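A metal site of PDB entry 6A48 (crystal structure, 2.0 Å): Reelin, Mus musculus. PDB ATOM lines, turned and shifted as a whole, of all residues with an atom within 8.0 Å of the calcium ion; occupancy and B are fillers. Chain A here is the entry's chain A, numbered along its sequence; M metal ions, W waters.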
ATOM      1  N   ASP A 169      -4.447  11.794  33.475  1.00  0.00           N
ATOM      2  CA  ASP A 169      -5.614  11.817  32.596  1.00  0.00           C
ATOM      3  C   ASP A 169      -5.717  13.194  31.955  1.00  0.00           C
ATOM      4  O   ASP A 169      -5.956  14.184  32.644  1.00  0.00           O
ATOM      5  CB  ASP A 169      -6.886  11.472  33.366  1.00  0.00           C
ATOM      6  CG  ASP A 169      -7.950  10.837  32.493  1.00  0.00           C
ATOM      7  OD1 ASP A 169      -7.988  11.127  31.278  1.00  0.00           O
ATOM      8  OD2 ASP A 169      -8.754  10.049  33.034  1.00  0.00           O
ATOM      9  N   ASN A 170      -5.537  13.254  30.630  1.00  0.00           N
ATOM     10  CA  ASN A 170      -5.829  14.447  29.860  1.00  0.00           C
ATOM     11  C   ASN A 170      -7.171  14.363  29.146  1.00  0.00           C
ATOM     12  O   ASN A 170      -7.439  15.154  28.236  1.00  0.00           O
ATOM     13  CB  ASN A 170      -4.708  14.714  28.845  1.00  0.00           C
ATOM     14  CG  ASN A 170      -4.563  13.601  27.828  1.00  0.00           C
ATOM     15  OD1 ASN A 170      -5.344  12.652  27.802  1.00  0.00           O
ATOM     16  ND2 ASN A 170      -3.547  13.714  26.974  1.00  0.00           N
ATOM     17  N   LEU A 171      -8.015  13.406  29.541  1.00  0.00           N
ATOM     18  CA  LEU A 171      -9.345  13.177  28.972  1.00  0.00           C
ATOM     19  C   LEU A 171      -9.297  12.817  27.488  1.00  0.00           C
ATOM     20  O   LEU A 171     -10.339  12.834  26.819  1.00  0.00           O
ATOM     21  CB  LEU A 171     -10.267  14.379  29.193  1.00  0.00           C
ATOM     22  CG  LEU A 171     -10.623  14.808  30.618  1.00  0.00           C
ATOM     23  CD1 LEU A 171     -10.964  13.602  31.480  1.00  0.00           C
ATOM     24  CD2 LEU A 171      -9.514  15.627  31.280  1.00  0.00           C
ATOM     25  N   ASP A 172      -8.131  12.493  26.949  1.00  0.00           N
ATOM     26  CA  ASP A 172      -8.000  12.207  25.529  1.00  0.00           C
ATOM     27  C   ASP A 172      -7.297  10.877  25.268  1.00  0.00           C
ATOM     28  O   ASP A 172      -6.153  10.863  24.810  1.00  0.00           O
ATOM     29  CB  ASP A 172      -7.241  13.333  24.817  1.00  0.00           C
ATOM     30  CG  ASP A 172      -7.909  14.682  24.973  1.00  0.00           C
ATOM     31  OD1 ASP A 172      -9.120  14.789  24.675  1.00  0.00           O
ATOM     32  OD2 ASP A 172      -7.229  15.634  25.387  1.00  0.00           O
ATOM     33  N   PRO A 173      -7.974   9.746  25.541  1.00  0.00           N
ATOM     34  CA  PRO A 173      -9.344   9.657  26.063  1.00  0.00           C
ATOM     35  C   PRO A 173      -9.366   9.594  27.585  1.00  0.00           C
ATOM     36  O   PRO A 173      -8.336   9.335  28.202  1.00  0.00           O
ATOM     37  CB  PRO A 173      -9.839   8.352  25.463  1.00  0.00           C
ATOM     38  CG  PRO A 173      -8.612   7.490  25.477  1.00  0.00           C
ATOM     39  CD  PRO A 173      -7.431   8.418  25.243  1.00  0.00           C
ATOM     40  N   VAL A 187     -17.382  15.178  30.133  1.00  0.00           N
ATOM     41  CA  VAL A 187     -16.108  15.052  29.439  1.00  0.00           C
ATOM     42  C   VAL A 187     -16.336  15.382  27.968  1.00  0.00           C
ATOM     43  O   VAL A 187     -17.006  14.623  27.254  1.00  0.00           O
ATOM     44  CB  VAL A 187     -15.494  13.658  29.595  1.00  0.00           C
ATOM     45  CG1 VAL A 187     -14.273  13.527  28.692  1.00  0.00           C
ATOM     46  CG2 VAL A 187     -15.110  13.406  31.044  1.00  0.00           C
ATOM     47  N   LYS A 188     -15.793  16.506  27.514  1.00  0.00           N
ATOM     48  CA  LYS A 188     -16.034  16.930  26.139  1.00  0.00           C
ATOM     49  C   LYS A 188     -15.057  18.033  25.780  1.00  0.00           C
ATOM     50  O   LYS A 188     -14.380  18.606  26.648  1.00  0.00           O
ATOM     51  CB  LYS A 188     -17.476  17.408  25.951  1.00  0.00           C
ATOM     52  CG  LYS A 188     -17.918  18.411  26.996  1.00  0.00           C
ATOM     53  CD  LYS A 188     -19.401  18.699  26.883  1.00  0.00           C
ATOM     54  CE  LYS A 188     -19.684  19.683  25.774  1.00  0.00           C
ATOM     55  NZ  LYS A 188     -19.540  21.091  26.212  1.00  0.00           N
ATOM     56  N   HIS A 189     -14.988  18.335  24.490  1.00  0.00           N
ATOM     57  CA  HIS A 189     -14.284  19.511  24.006  1.00  0.00           C
ATOM     58  C   HIS A 189     -15.174  20.727  24.202  1.00  0.00           C
ATOM     59  O   HIS A 189     -16.265  20.807  23.615  1.00  0.00           O
ATOM     60  CB  HIS A 189     -13.888  19.346  22.534  1.00  0.00           C
ATOM     61  CG  HIS A 189     -13.254  20.568  21.945  1.00  0.00           C
ATOM     62  ND1 HIS A 189     -12.000  21.007  22.304  1.00  0.00           N
ATOM     63  CD2 HIS A 189     -13.720  21.456  21.036  1.00  0.00           C
ATOM     64  CE1 HIS A 189     -11.705  22.104  21.630  1.00  0.00           C
ATOM     65  NE2 HIS A 189     -12.733  22.397  20.847  1.00  0.00           N
ATOM     66  N   SER A 193     -10.666  23.884  25.233  1.00  0.00           N
ATOM     67  CA  SER A 193      -9.730  22.944  25.832  1.00  0.00           C
ATOM     68  C   SER A 193      -8.862  22.283  24.762  1.00  0.00           C
ATOM     69  O   SER A 193      -9.196  22.258  23.573  1.00  0.00           O
ATOM     70  CB  SER A 193     -10.485  21.880  26.632  1.00  0.00           C
ATOM     71  OG  SER A 193     -11.245  21.046  25.782  1.00  0.00           O
ATOM     72  N   ASP A 194      -7.725  21.744  25.207  1.00  0.00           N
ATOM     73  CA  ASP A 194      -6.896  20.881  24.380  1.00  0.00           C
ATOM     74  C   ASP A 194      -7.570  19.514  24.327  1.00  0.00           C
ATOM     75  O   ASP A 194      -7.471  18.721  25.272  1.00  0.00           O
ATOM     76  CB  ASP A 194      -5.480  20.786  24.944  1.00  0.00           C
ATOM     77  CG  ASP A 194      -4.619  19.778  24.206  1.00  0.00           C
ATOM     78  OD1 ASP A 194      -4.751  19.658  22.974  1.00  0.00           O
ATOM     79  OD2 ASP A 194      -3.803  19.100  24.865  1.00  0.00           O
ATOM     80  N   GLY A 195      -8.268  19.233  23.232  1.00  0.00           N
ATOM     81  CA  GLY A 195      -9.070  18.027  23.173  1.00  0.00           C
ATOM     82  C   GLY A 195     -10.218  18.083  24.157  1.00  0.00           C
ATOM     83  O   GLY A 195     -10.901  19.109  24.301  1.00  0.00           O
ATOM     84  N   ASN A 196     -10.441  16.979  24.861  1.00  0.00           N
ATOM     85  CA  ASN A 196     -11.476  16.930  25.875  1.00  0.00           C
ATOM     86  C   ASN A 196     -10.976  17.511  27.195  1.00  0.00           C
ATOM     87  O   ASN A 196      -9.782  17.501  27.488  1.00  0.00           O
ATOM     88  CB  ASN A 196     -11.942  15.486  26.107  1.00  0.00           C
ATOM     89  CG  ASN A 196     -12.601  14.890  24.890  1.00  0.00           C
ATOM     90  OD1 ASN A 196     -13.463  15.506  24.257  1.00  0.00           O
ATOM     91  ND2 ASN A 196     -12.196  13.672  24.531  1.00  0.00           N
ATOM     92  N   SER A 197     -11.919  18.014  27.980  1.00  0.00           N
ATOM     93  CA  SER A 197     -11.667  18.379  29.372  1.00  0.00           C
ATOM     94  C   SER A 197     -12.897  17.966  30.186  1.00  0.00           C
ATOM     95  O   SER A 197     -13.889  17.478  29.652  1.00  0.00           O
ATOM     96  CB  SER A 197     -11.381  19.874  29.512  1.00  0.00           C
ATOM     97  OG  SER A 197     -12.452  20.661  29.009  1.00  0.00           O
ATOM     98  N   ILE A 198     -12.804  18.156  31.505  1.00  0.00           N
ATOM     99  CA  ILE A 198     -13.944  17.984  32.385  1.00  0.00           C
ATOM    100  C   ILE A 198     -14.603  19.344  32.509  1.00  0.00           C
ATOM    101  O   ILE A 198     -14.087  20.240  33.194  1.00  0.00           O
ATOM    102  CB  ILE A 198     -13.535  17.432  33.751  1.00  0.00           C
ATOM    103  CG1 ILE A 198     -12.897  16.054  33.601  1.00  0.00           C
ATOM    104  CG2 ILE A 198     -14.737  17.393  34.697  1.00  0.00           C
ATOM    105  CD1 ILE A 198     -12.346  15.487  34.900  1.00  0.00           C
ATOM    106  N   TRP A 439      -6.829  29.508  30.341  1.00  0.00           N
ATOM    107  CA  TRP A 439      -6.290  28.273  30.882  1.00  0.00           C
ATOM    108  C   TRP A 439      -4.992  28.523  31.641  1.00  0.00           C
ATOM    109  O   TRP A 439      -4.110  29.242  31.166  1.00  0.00           O
ATOM    110  CB  TRP A 439      -6.052  27.253  29.766  1.00  0.00           C
ATOM    111  CG  TRP A 439      -7.293  26.556  29.332  1.00  0.00           C
ATOM    112  CD1 TRP A 439      -8.069  26.869  28.250  1.00  0.00           C
ATOM    113  CD2 TRP A 439      -7.908  25.435  29.964  1.00  0.00           C
ATOM    114  NE1 TRP A 439      -9.129  25.999  28.171  1.00  0.00           N
ATOM    115  CE2 TRP A 439      -9.056  25.102  29.209  1.00  0.00           C
ATOM    116  CE3 TRP A 439      -7.601  24.659  31.095  1.00  0.00           C
ATOM    117  CZ2 TRP A 439      -9.891  24.051  29.551  1.00  0.00           C
ATOM    118  CZ3 TRP A 439      -8.442  23.609  31.430  1.00  0.00           C
ATOM    119  CH2 TRP A 439      -9.573  23.309  30.654  1.00  0.00           C
ATOM    120  N   ILE A 472     -11.341  21.537  33.941  1.00  0.00           N
ATOM    121  CA  ILE A 472     -10.003  21.076  34.299  1.00  0.00           C
ATOM    122  C   ILE A 472      -9.525  20.098  33.241  1.00  0.00           C
ATOM    123  O   ILE A 472     -10.333  19.467  32.550  1.00  0.00           O
ATOM    124  CB  ILE A 472      -9.950  20.422  35.705  1.00  0.00           C
ATOM    125  CG1 ILE A 472     -10.883  19.215  35.769  1.00  0.00           C
ATOM    126  CG2 ILE A 472     -10.287  21.441  36.799  1.00  0.00           C
ATOM    127  CD1 ILE A 472     -10.829  18.476  37.092  1.00  0.00           C
ATOM    128  N   ASP A 473      -8.215  19.962  33.134  1.00  0.00           N
ATOM    129  CA  ASP A 473      -7.590  19.154  32.093  1.00  0.00           C
ATOM    130  C   ASP A 473      -6.187  18.776  32.571  1.00  0.00           C
ATOM    131  O   ASP A 473      -5.705  19.311  33.568  1.00  0.00           O
ATOM    132  CB  ASP A 473      -7.542  19.907  30.752  1.00  0.00           C
ATOM    133  CG  ASP A 473      -7.433  18.977  29.552  1.00  0.00           C
ATOM    134  OD1 ASP A 473      -7.242  17.760  29.741  1.00  0.00           O
ATOM    135  OD2 ASP A 473      -7.544  19.464  28.410  1.00  0.00           O
ATOM    136  N   ASN A 474      -5.566  17.843  31.852  1.00  0.00           N
ATOM    137  CA  ASN A 474      -4.148  17.502  32.048  1.00  0.00           C
ATOM    138  C   ASN A 474      -3.821  17.213  33.511  1.00  0.00           C
ATOM    139  O   ASN A 474      -2.889  17.783  34.085  1.00  0.00           O
ATOM    140  CB  ASN A 474      -3.256  18.631  31.502  1.00  0.00           C
ATOM    141  CG  ASN A 474      -3.482  18.879  30.026  1.00  0.00           C
ATOM    142  OD1 ASN A 474      -3.782  17.945  29.272  1.00  0.00           O
ATOM    143  ND2 ASN A 474      -3.346  20.129  29.609  1.00  0.00           N
ATOM    144  N   VAL A 475      -4.592  16.307  34.105  1.00  0.00           N
ATOM    145  CA  VAL A 475      -4.425  15.985  35.524  1.00  0.00           C
ATOM    146  C   VAL A 475      -3.293  14.986  35.695  1.00  0.00           C
ATOM    147  O   VAL A 475      -3.231  13.968  35.004  1.00  0.00           O
ATOM    148  CB  VAL A 475      -5.737  15.429  36.114  1.00  0.00           C
ATOM    149  CG1 VAL A 475      -5.510  14.930  37.526  1.00  0.00           C
ATOM    150  CG2 VAL A 475      -6.836  16.495  36.073  1.00  0.00           C
HETATM  151 CA    CA M   1      -7.480  17.255  27.201  1.00  0.00          CA
HETATM  152  O   HOH W   1      -5.195  17.846  27.044  1.00  0.00           O
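Five residues have an atom within 4 Å of the calcium ion: Asn 170, Asp 172, Asp 194, Asn 196 and Asp 473.
Water W1 lies within hydrogen-bond range of OD1 of Asn 474 and OD2 of Asp 194.
The calcium ion is bound by the backbone carbonyl oxygen (O) of Asn 196, the backbone carbonyl oxygen (O) of Asn 170, water W1, the backbone carbonyl oxygen (O) of Asp 194, the side-chain carboxylate (OD2) of Asp 172, the side-chain carboxylate (OD2) of Asp 473 and the side-chain carboxylate (OD1) of Asp 473.
ND2 of Asn 196 is in hydrogen-bond range of O of Leu 171 (3.1 Å).
OD1 of Asn 196 sits at hydrogen-bond distance from N of His 189.
OD1 of Asp 473 sits close to OD1 of Asn 474, 3.5 Å away.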
